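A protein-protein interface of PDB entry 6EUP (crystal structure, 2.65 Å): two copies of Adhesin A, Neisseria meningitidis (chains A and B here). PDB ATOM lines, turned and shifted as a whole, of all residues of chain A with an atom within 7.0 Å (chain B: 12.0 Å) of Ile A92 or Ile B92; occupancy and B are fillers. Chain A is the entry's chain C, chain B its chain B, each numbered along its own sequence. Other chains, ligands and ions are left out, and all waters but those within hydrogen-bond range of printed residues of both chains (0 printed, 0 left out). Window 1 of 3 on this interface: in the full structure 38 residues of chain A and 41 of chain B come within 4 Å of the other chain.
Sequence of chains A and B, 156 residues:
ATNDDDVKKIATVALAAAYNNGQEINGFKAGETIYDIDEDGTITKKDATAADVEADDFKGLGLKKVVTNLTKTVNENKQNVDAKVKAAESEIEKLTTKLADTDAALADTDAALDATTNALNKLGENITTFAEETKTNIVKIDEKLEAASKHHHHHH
Of chain A, only Ala A88, Glu A91, Ile A92 and Leu A95 come within 4 Å of Ile B92. Ala A88 touches two residues of chain B. Ser A90 touches none of the printed residues of chain B. Printed residues of chain B within 4 Å of Glu A91: Glu B89 (3.0 Å) and Ile B92 (3.6 Å). Glu A93 touches none of the printed residues of chain B. Of chain B, only Ile B92 (3.9 Å), Thr B96 (3.8 Å) and Leu B99 (3.8 Å) come within 4 Å of Leu A95. No residue of chain B comes within 4 Å of Thr A96. Of the printed residues of chain A, Leu B99 touches Leu A95 (3.8 Å). Of the printed residues of chain A, Glu B89 touches Ala A88 and Glu A91. The nearest residue of chain B that does not touch Ile A92 is Ala B88 (6.5 Å). The nearest residue of chain A that does not touch Ile B92 is Glu A89 (5.5 Å). The nearest printed residue of chain A that does not touch Thr B96 is Glu A91 (6.2 Å).
The backbone carbonyl oxygen (O) of Ile A92 is in hydrogen-bond range of the side-chain hydroxyl (OG1) of Thr A96 (2.8 Å). The side-chain hydroxyl of Thr B96 lies within hydrogen-bond range of the backbone carbonyl oxygen of Ile B92 (2.8 Å).
Ala A88 touches Glu B89, but with the chains exchanged Glu A89 does not touch Ala B88 (8.0 Å). Ala A88 touches Ile B92, but with the chains exchanged Ile A92 does not touch Ala B88 (6.5 Å). Glu A91 touches Ile B92, but with the chains exchanged Ile A92 does not touch Glu B91 (7.8 Å). Leu A95 touches Thr B96, but with the chains exchanged Thr A96 does not touch Leu B95 (8.4 Å). 12 positions are printed for both chains.
Ala A88 touches Glu B89. CD1 of Ile B92 touches O of Ala A88 (3.7 Å). Glu A91 touches Ile B92 (OE2 to CG2, 3.6 Å). CD1 of Ile B92 touches CG1 of Ile A92, at 3.9 Å. Leu A95 touches Ile B92. Leu A95 touches Thr B96. Leu B99 touches Leu A95 (CD2 to CD2, 3.8 Å).
The side-chain carboxylate of Glu A91 sits close to the side-chain carboxylate of Glu B89, at 3.0 Å.
Of the 21 printed residues of chain B, 4 touch a printed residue of chain A. Hydrophobic or aromatic side chains of chain B within 4 Å of the printed part of chain A: Ile B92 and Leu B99. Of the 12 printed residues of chain A, 4 touch a printed residue of chain B. Hydrophobic or aromatic side chains of chain A that line the printed part of chain B: Ala A88, Ile A92 and Leu A95. Among the printed residues, 8 pairs touch across the chains.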
ATOM      1  N   VAL A  85     -29.986  13.929 -15.597  1.00  0.00           N
ATOM      2  CA  VAL A  85     -28.625  14.010 -16.134  1.00  0.00           C
ATOM      3  C   VAL A  85     -28.654  13.833 -17.665  1.00  0.00           C
ATOM      4  O   VAL A  85     -27.927  14.543 -18.366  1.00  0.00           O
ATOM      5  CB  VAL A  85     -27.643  13.056 -15.388  1.00  0.00           C
ATOM      6  CG1 VAL A  85     -26.305  12.928 -16.109  1.00  0.00           C
ATOM      7  CG2 VAL A  85     -27.418  13.525 -13.951  1.00  0.00           C
ATOM      8  N   ALA A  87     -31.120  14.757 -19.521  1.00  0.00           N
ATOM      9  CA  ALA A  87     -31.750  16.009 -19.935  1.00  0.00           C
ATOM     10  C   ALA A  87     -30.707  17.131 -19.977  1.00  0.00           C
ATOM     11  O   ALA A  87     -30.696  17.910 -20.930  1.00  0.00           O
ATOM     12  CB  ALA A  87     -32.874  16.375 -18.982  1.00  0.00           C
ATOM     13  N   ALA A  88     -29.832  17.197 -18.953  1.00  0.00           N
ATOM     14  CA  ALA A  88     -28.756  18.181 -18.849  1.00  0.00           C
ATOM     15  C   ALA A  88     -27.758  17.980 -19.988  1.00  0.00           C
ATOM     16  O   ALA A  88     -27.370  18.955 -20.631  1.00  0.00           O
ATOM     17  CB  ALA A  88     -28.054  18.054 -17.503  1.00  0.00           C
ATOM     18  N   GLU A  89     -27.386  16.714 -20.267  1.00  0.00           N
ATOM     19  CA  GLU A  89     -26.463  16.361 -21.343  1.00  0.00           C
ATOM     20  C   GLU A  89     -27.041  16.684 -22.722  1.00  0.00           C
ATOM     21  O   GLU A  89     -26.278  16.982 -23.648  1.00  0.00           O
ATOM     22  CB  GLU A  89     -26.090  14.885 -21.263  1.00  0.00           C
ATOM     23  CG  GLU A  89     -24.921  14.606 -20.339  1.00  0.00           C
ATOM     24  CD  GLU A  89     -23.794  13.857 -21.028  1.00  0.00           C
ATOM     25  OE1 GLU A  89     -23.722  12.614 -20.871  1.00  0.00           O
ATOM     26  OE2 GLU A  89     -22.942  14.510 -21.675  1.00  0.00           O
ATOM     27  N   SER A  90     -28.385  16.615 -22.860  1.00  0.00           N
ATOM     28  CA  SER A  90     -29.106  16.927 -24.095  1.00  0.00           C
ATOM     29  C   SER A  90     -28.995  18.430 -24.364  1.00  0.00           C
ATOM     30  O   SER A  90     -28.779  18.828 -25.511  1.00  0.00           O
ATOM     31  CB  SER A  90     -30.571  16.516 -23.981  1.00  0.00           C
ATOM     32  OG  SER A  90     -31.276  16.745 -25.190  1.00  0.00           O
ATOM     33  N   GLU A  91     -29.110  19.255 -23.299  1.00  0.00           N
ATOM     34  CA  GLU A  91     -28.979  20.705 -23.374  1.00  0.00           C
ATOM     35  C   GLU A  91     -27.542  21.040 -23.761  1.00  0.00           C
ATOM     36  O   GLU A  91     -27.331  21.753 -24.745  1.00  0.00           O
ATOM     37  CB  GLU A  91     -29.397  21.370 -22.054  1.00  0.00           C
ATOM     38  CG  GLU A  91     -30.907  21.494 -21.896  1.00  0.00           C
ATOM     39  CD  GLU A  91     -31.445  21.496 -20.474  1.00  0.00           C
ATOM     40  OE1 GLU A  91     -31.985  20.450 -20.042  1.00  0.00           O
ATOM     41  OE2 GLU A  91     -31.379  22.559 -19.814  1.00  0.00           O
ATOM     42  N   ILE A  92     -26.563  20.418 -23.079  1.00  0.00           N
ATOM     43  CA  ILE A  92     -25.137  20.588 -23.368  1.00  0.00           C
ATOM     44  C   ILE A  92     -24.840  20.254 -24.835  1.00  0.00           C
ATOM     45  O   ILE A  92     -24.083  20.981 -25.472  1.00  0.00           O
ATOM     46  CB  ILE A  92     -24.235  19.805 -22.363  1.00  0.00           C
ATOM     47  CG1 ILE A  92     -24.363  20.400 -20.944  1.00  0.00           C
ATOM     48  CG2 ILE A  92     -22.766  19.785 -22.813  1.00  0.00           C
ATOM     49  CD1 ILE A  92     -23.921  19.477 -19.798  1.00  0.00           C
ATOM     50  N   GLU A  93     -25.455  19.197 -25.374  1.00  0.00           N
ATOM     51  CA  GLU A  93     -25.249  18.801 -26.764  1.00  0.00           C
ATOM     52  C   GLU A  93     -25.798  19.860 -27.749  1.00  0.00           C
ATOM     53  O   GLU A  93     -25.155  20.127 -28.778  1.00  0.00           O
ATOM     54  CB  GLU A  93     -25.836  17.395 -27.013  1.00  0.00           C
ATOM     55  CG  GLU A  93     -25.810  16.911 -28.455  1.00  0.00           C
ATOM     56  CD  GLU A  93     -24.473  16.493 -29.041  1.00  0.00           C
ATOM     57  OE1 GLU A  93     -23.886  15.501 -28.545  1.00  0.00           O
ATOM     58  OE2 GLU A  93     -24.049  17.113 -30.046  1.00  0.00           O
ATOM     59  N   LYS A  94     -26.954  20.473 -27.417  1.00  0.00           N
ATOM     60  CA  LYS A  94     -27.570  21.501 -28.255  1.00  0.00           C
ATOM     61  C   LYS A  94     -26.753  22.800 -28.233  1.00  0.00           C
ATOM     62  O   LYS A  94     -26.531  23.389 -29.296  1.00  0.00           O
ATOM     63  CB  LYS A  94     -29.055  21.713 -27.914  1.00  0.00           C
ATOM     64  CG  LYS A  94     -29.949  20.662 -28.560  1.00  0.00           C
ATOM     65  CD  LYS A  94     -31.427  20.818 -28.215  1.00  0.00           C
ATOM     66  CE  LYS A  94     -32.262  19.627 -28.665  1.00  0.00           C
ATOM     67  NZ  LYS A  94     -32.214  18.478 -27.715  1.00  0.00           N
ATOM     68  N   LEU A  95     -26.246  23.193 -27.038  1.00  0.00           N
ATOM     69  CA  LEU A  95     -25.401  24.372 -26.849  1.00  0.00           C
ATOM     70  C   LEU A  95     -24.116  24.231 -27.650  1.00  0.00           C
ATOM     71  O   LEU A  95     -23.711  25.191 -28.291  1.00  0.00           O
ATOM     72  CB  LEU A  95     -25.064  24.601 -25.367  1.00  0.00           C
ATOM     73  CG  LEU A  95     -26.100  25.358 -24.546  1.00  0.00           C
ATOM     74  CD1 LEU A  95     -25.904  25.091 -23.071  1.00  0.00           C
ATOM     75  CD2 LEU A  95     -26.029  26.857 -24.799  1.00  0.00           C
ATOM     76  N   THR A  96     -23.501  23.033 -27.647  1.00  0.00           N
ATOM     77  CA  THR A  96     -22.269  22.729 -28.392  1.00  0.00           C
ATOM     78  C   THR A  96     -22.460  22.947 -29.909  1.00  0.00           C
ATOM     79  O   THR A  96     -21.614  23.573 -30.552  1.00  0.00           O
ATOM     80  CB  THR A  96     -21.766  21.322 -28.028  1.00  0.00           C
ATOM     81  OG1 THR A  96     -21.575  21.261 -26.614  1.00  0.00           O
ATOM     82  CG2 THR A  96     -20.454  20.961 -28.719  1.00  0.00           C
ATOM     83  N   THR A  97     -23.575  22.449 -30.462  1.00  0.00           N
ATOM     84  CA  THR A  97     -23.886  22.591 -31.883  1.00  0.00           C
ATOM     85  C   THR A  97     -24.099  24.070 -32.236  1.00  0.00           C
ATOM     86  O   THR A  97     -23.555  24.537 -33.230  1.00  0.00           O
ATOM     87  CB  THR A  97     -25.053  21.660 -32.283  1.00  0.00           C
ATOM     88  OG1 THR A  97     -24.703  20.306 -31.981  1.00  0.00           O
ATOM     89  CG2 THR A  97     -25.404  21.758 -33.765  1.00  0.00           C
ATOM     90  N   VAL B  81     -27.423  15.175  -4.697  1.00  0.00           N
ATOM     91  CA  VAL B  81     -27.395  15.136  -6.150  1.00  0.00           C
ATOM     92  C   VAL B  81     -28.424  16.107  -6.774  1.00  0.00           C
ATOM     93  O   VAL B  81     -28.112  16.711  -7.803  1.00  0.00           O
ATOM     94  CB  VAL B  81     -27.474  13.707  -6.736  1.00  0.00           C
ATOM     95  CG1 VAL B  81     -28.899  13.169  -6.746  1.00  0.00           C
ATOM     96  CG2 VAL B  81     -26.871  13.668  -8.139  1.00  0.00           C
ATOM     97  N   ASP B  82     -29.601  16.302  -6.149  1.00  0.00           N
ATOM     98  CA  ASP B  82     -30.612  17.233  -6.672  1.00  0.00           C
ATOM     99  C   ASP B  82     -30.084  18.681  -6.714  1.00  0.00           C
ATOM    100  O   ASP B  82     -30.406  19.419  -7.647  1.00  0.00           O
ATOM    101  CB  ASP B  82     -31.932  17.161  -5.876  1.00  0.00           C
ATOM    102  CG  ASP B  82     -32.770  15.898  -6.057  1.00  0.00           C
ATOM    103  OD1 ASP B  82     -32.453  15.091  -6.966  1.00  0.00           O
ATOM    104  OD2 ASP B  82     -33.744  15.716  -5.287  1.00  0.00           O
ATOM    105  N   ALA B  83     -29.258  19.062  -5.717  1.00  0.00           N
ATOM    106  CA  ALA B  83     -28.648  20.381  -5.616  1.00  0.00           C
ATOM    107  C   ALA B  83     -27.556  20.545  -6.669  1.00  0.00           C
ATOM    108  O   ALA B  83     -27.420  21.635  -7.230  1.00  0.00           O
ATOM    109  CB  ALA B  83     -28.079  20.598  -4.227  1.00  0.00           C
ATOM    110  N   LYS B  84     -26.794  19.462  -6.950  1.00  0.00           N
ATOM    111  CA  LYS B  84     -25.730  19.465  -7.956  1.00  0.00           C
ATOM    112  C   LYS B  84     -26.330  19.625  -9.358  1.00  0.00           C
ATOM    113  O   LYS B  84     -25.805  20.402 -10.158  1.00  0.00           O
ATOM    114  CB  LYS B  84     -24.888  18.184  -7.873  1.00  0.00           C
ATOM    115  CG  LYS B  84     -23.822  18.225  -6.791  1.00  0.00           C
ATOM    116  CD  LYS B  84     -23.125  16.875  -6.608  1.00  0.00           C
ATOM    117  CE  LYS B  84     -22.144  16.916  -5.460  1.00  0.00           C
ATOM    118  NZ  LYS B  84     -21.449  15.623  -5.279  1.00  0.00           N
ATOM    119  N   VAL B  85     -27.443  18.909  -9.635  1.00  0.00           N
ATOM    120  CA  VAL B  85     -28.165  18.946 -10.915  1.00  0.00           C
ATOM    121  C   VAL B  85     -28.861  20.309 -11.089  1.00  0.00           C
ATOM    122  O   VAL B  85     -28.841  20.856 -12.198  1.00  0.00           O
ATOM    123  CB  VAL B  85     -29.103  17.713 -11.086  1.00  0.00           C
ATOM    124  CG1 VAL B  85     -30.083  17.880 -12.248  1.00  0.00           C
ATOM    125  CG2 VAL B  85     -28.286  16.432 -11.256  1.00  0.00           C
ATOM    126  N   LYS B  86     -29.406  20.886  -9.996  1.00  0.00           N
ATOM    127  CA  LYS B  86     -30.036  22.205 -10.049  1.00  0.00           C
ATOM    128  C   LYS B  86     -28.971  23.298 -10.333  1.00  0.00           C
ATOM    129  O   LYS B  86     -29.272  24.302 -10.999  1.00  0.00           O
ATOM    130  CB  LYS B  86     -30.810  22.512  -8.764  1.00  0.00           C
ATOM    131  CG  LYS B  86     -32.063  23.334  -9.026  1.00  0.00           C
ATOM    132  CD  LYS B  86     -32.721  23.827  -7.749  1.00  0.00           C
ATOM    133  CE  LYS B  86     -34.088  24.426  -8.008  1.00  0.00           C
ATOM    134  NZ  LYS B  86     -34.850  24.649  -6.743  1.00  0.00           N
ATOM    135  N   ALA B  87     -27.720  23.066  -9.851  1.00  0.00           N
ATOM    136  CA  ALA B  87     -26.571  23.946 -10.045  1.00  0.00           C
ATOM    137  C   ALA B  87     -26.106  23.880 -11.493  1.00  0.00           C
ATOM    138  O   ALA B  87     -25.812  24.926 -12.079  1.00  0.00           O
ATOM    139  CB  ALA B  87     -25.436  23.548  -9.120  1.00  0.00           C
ATOM    140  N   ALA B  88     -26.041  22.653 -12.067  1.00  0.00           N
ATOM    141  CA  ALA B  88     -25.634  22.403 -13.449  1.00  0.00           C
ATOM    142  C   ALA B  88     -26.635  23.050 -14.402  1.00  0.00           C
ATOM    143  O   ALA B  88     -26.221  23.718 -15.349  1.00  0.00           O
ATOM    144  CB  ALA B  88     -25.537  20.908 -13.712  1.00  0.00           C
ATOM    145  N   GLU B  89     -27.943  22.901 -14.117  1.00  0.00           N
ATOM    146  CA  GLU B  89     -29.015  23.484 -14.920  1.00  0.00           C
ATOM    147  C   GLU B  89     -28.996  25.012 -14.872  1.00  0.00           C
ATOM    148  O   GLU B  89     -29.389  25.655 -15.846  1.00  0.00           O
ATOM    149  CB  GLU B  89     -30.381  22.948 -14.477  1.00  0.00           C
ATOM    150  CG  GLU B  89     -30.760  21.617 -15.110  1.00  0.00           C
ATOM    151  CD  GLU B  89     -31.071  21.650 -16.598  1.00  0.00           C
ATOM    152  OE1 GLU B  89     -30.175  21.281 -17.391  1.00  0.00           O
ATOM    153  OE2 GLU B  89     -32.172  22.115 -16.972  1.00  0.00           O
ATOM    154  N   SER B  90     -28.549  25.588 -13.737  1.00  0.00           N
ATOM    155  CA  SER B  90     -28.427  27.032 -13.544  1.00  0.00           C
ATOM    156  C   SER B  90     -27.322  27.564 -14.476  1.00  0.00           C
ATOM    157  O   SER B  90     -27.491  28.617 -15.096  1.00  0.00           O
ATOM    158  CB  SER B  90     -28.103  27.350 -12.087  1.00  0.00           C
ATOM    159  OG  SER B  90     -28.018  28.748 -11.862  1.00  0.00           O
ATOM    160  N   GLU B  91     -26.223  26.792 -14.597  1.00  0.00           N
ATOM    161  CA  GLU B  91     -25.073  27.081 -15.434  1.00  0.00           C
ATOM    162  C   GLU B  91     -25.472  27.009 -16.897  1.00  0.00           C
ATOM    163  O   GLU B  91     -25.152  27.927 -17.658  1.00  0.00           O
ATOM    164  CB  GLU B  91     -23.910  26.142 -15.101  1.00  0.00           C
ATOM    165  CG  GLU B  91     -23.242  26.508 -13.783  1.00  0.00           C
ATOM    166  CD  GLU B  91     -22.343  25.467 -13.144  1.00  0.00           C
ATOM    167  OE1 GLU B  91     -21.153  25.391 -13.532  1.00  0.00           O
ATOM    168  OE2 GLU B  91     -22.800  24.791 -12.191  1.00  0.00           O
ATOM    169  N   ILE B  92     -26.245  25.974 -17.267  1.00  0.00           N
ATOM    170  CA  ILE B  92     -26.787  25.770 -18.611  1.00  0.00           C
ATOM    171  C   ILE B  92     -27.730  26.918 -18.985  1.00  0.00           C
ATOM    172  O   ILE B  92     -27.686  27.384 -20.119  1.00  0.00           O
ATOM    173  CB  ILE B  92     -27.448  24.366 -18.757  1.00  0.00           C
ATOM    174  CG1 ILE B  92     -26.386  23.247 -18.648  1.00  0.00           C
ATOM    175  CG2 ILE B  92     -28.253  24.241 -20.069  1.00  0.00           C
ATOM    176  CD1 ILE B  92     -26.933  21.852 -18.324  1.00  0.00           C
ATOM    177  N   GLU B  93     -28.542  27.393 -18.036  1.00  0.00           N
ATOM    178  CA  GLU B  93     -29.491  28.492 -18.276  1.00  0.00           C
ATOM    179  C   GLU B  93     -28.754  29.817 -18.566  1.00  0.00           C
ATOM    180  O   GLU B  93     -29.182  30.575 -19.451  1.00  0.00           O
ATOM    181  CB  GLU B  93     -30.490  28.650 -17.100  1.00  0.00           C
ATOM    182  CG  GLU B  93     -31.924  28.156 -17.345  1.00  0.00           C
ATOM    183  CD  GLU B  93     -32.514  27.243 -16.274  1.00  0.00           C
ATOM    184  OE1 GLU B  93     -32.576  27.660 -15.093  1.00  0.00           O
ATOM    185  OE2 GLU B  93     -32.938  26.116 -16.624  1.00  0.00           O
ATOM    186  N   LYS B  94     -27.634  30.069 -17.845  1.00  0.00           N
ATOM    187  CA  LYS B  94     -26.833  31.275 -18.038  1.00  0.00           C
ATOM    188  C   LYS B  94     -26.087  31.254 -19.391  1.00  0.00           C
ATOM    189  O   LYS B  94     -26.075  32.275 -20.091  1.00  0.00           O
ATOM    190  CB  LYS B  94     -25.904  31.546 -16.848  1.00  0.00           C
ATOM    191  CG  LYS B  94     -26.621  32.199 -15.664  1.00  0.00           C
ATOM    192  CD  LYS B  94     -25.679  32.483 -14.495  1.00  0.00           C
ATOM    193  CE  LYS B  94     -26.394  32.808 -13.200  1.00  0.00           C
ATOM    194  NZ  LYS B  94     -26.560  31.597 -12.343  1.00  0.00           N
ATOM    195  N   LEU B  95     -25.540  30.069 -19.783  1.00  0.00           N
ATOM    196  CA  LEU B  95     -24.851  29.866 -21.052  1.00  0.00           C
ATOM    197  C   LEU B  95     -25.803  30.110 -22.210  1.00  0.00           C
ATOM    198  O   LEU B  95     -25.416  30.767 -23.174  1.00  0.00           O
ATOM    199  CB  LEU B  95     -24.262  28.455 -21.152  1.00  0.00           C
ATOM    200  CG  LEU B  95     -22.891  28.241 -20.515  1.00  0.00           C
ATOM    201  CD1 LEU B  95     -22.651  26.768 -20.225  1.00  0.00           C
ATOM    202  CD2 LEU B  95     -21.767  28.790 -21.399  1.00  0.00           C
ATOM    203  N   THR B  96     -27.054  29.621 -22.105  1.00  0.00           N
ATOM    204  CA  THR B  96     -28.105  29.791 -23.121  1.00  0.00           C
ATOM    205  C   THR B  96     -28.401  31.286 -23.382  1.00  0.00           C
ATOM    206  O   THR B  96     -28.478  31.709 -24.538  1.00  0.00           O
ATOM    207  CB  THR B  96     -29.354  28.973 -22.733  1.00  0.00           C
ATOM    208  OG1 THR B  96     -28.970  27.606 -22.586  1.00  0.00           O
ATOM    209  CG2 THR B  96     -30.462  29.052 -23.769  1.00  0.00           C
ATOM    210  N   THR B  97     -28.546  32.072 -22.305  1.00  0.00           N
ATOM    211  CA  THR B  97     -28.823  33.505 -22.397  1.00  0.00           C
ATOM    212  C   THR B  97     -27.640  34.230 -23.058  1.00  0.00           C
ATOM    213  O   THR B  97     -27.860  35.050 -23.942  1.00  0.00           O
ATOM    214  CB  THR B  97     -29.233  34.068 -21.014  1.00  0.00           C
ATOM    215  OG1 THR B  97     -30.396  33.379 -20.564  1.00  0.00           O
ATOM    216  CG2 THR B  97     -29.530  35.561 -21.046  1.00  0.00           C
ATOM    217  N   LYS B  98     -26.401  33.885 -22.658  1.00  0.00           N
ATOM    218  CA  LYS B  98     -25.180  34.485 -23.188  1.00  0.00           C
ATOM    219  C   LYS B  98     -24.934  34.106 -24.625  1.00  0.00           C
ATOM    220  O   LYS B  98     -24.408  34.930 -25.370  1.00  0.00           O
ATOM    221  CB  LYS B  98     -23.948  34.168 -22.317  1.00  0.00           C
ATOM    222  CG  LYS B  98     -23.221  35.412 -21.787  1.00  0.00           C
ATOM    223  CD  LYS B  98     -22.446  36.173 -22.875  1.00  0.00           C
ATOM    224  CE  LYS B  98     -22.153  37.605 -22.500  1.00  0.00           C
ATOM    225  NZ  LYS B  98     -23.329  38.489 -22.719  1.00  0.00           N
ATOM    226  N   LEU B  99     -25.320  32.880 -25.030  1.00  0.00           N
ATOM    227  CA  LEU B  99     -25.175  32.439 -26.416  1.00  0.00           C
ATOM    228  C   LEU B  99     -26.214  33.130 -27.320  1.00  0.00           C
ATOM    229  O   LEU B  99     -25.923  33.406 -28.485  1.00  0.00           O
ATOM    230  CB  LEU B  99     -25.217  30.900 -26.548  1.00  0.00           C
ATOM    231  CG  LEU B  99     -24.935  30.291 -27.941  1.00  0.00           C
ATOM    232  CD1 LEU B  99     -23.600  30.771 -28.509  1.00  0.00           C
ATOM    233  CD2 LEU B  99     -24.941  28.782 -27.885  1.00  0.00           C
ATOM    234  N   ALA B 100     -27.401  33.435 -26.773  1.00  0.00           N
ATOM    235  CA  ALA B 100     -28.455  34.122 -27.514  1.00  0.00           C
ATOM    236  C   ALA B 100     -28.102  35.619 -27.689  1.00  0.00           C
ATOM    237  O   ALA B 100     -28.448  36.217 -28.712  1.00  0.00           O
ATOM    238  CB  ALA B 100     -29.785  33.964 -26.804  1.00  0.00           C
ATOM    239  N   ASP B 101     -27.387  36.198 -26.696  1.00  0.00           N
ATOM    240  CA  ASP B 101     -26.914  37.577 -26.695  1.00  0.00           C
ATOM    241  C   ASP B 101     -25.765  37.752 -27.710  1.00  0.00           C
ATOM    242  O   ASP B 101     -25.686  38.799 -28.355  1.00  0.00           O
ATOM    243  CB  ASP B 101     -26.470  37.993 -25.283  1.00  0.00           C
ATOM    244  CG  ASP B 101     -27.612  38.284 -24.316  1.00  0.00           C
ATOM    245  OD1 ASP B 101     -28.639  38.853 -24.761  1.00  0.00           O
ATOM    246  OD2 ASP B 101     -27.458  37.987 -23.095  1.00  0.00           O
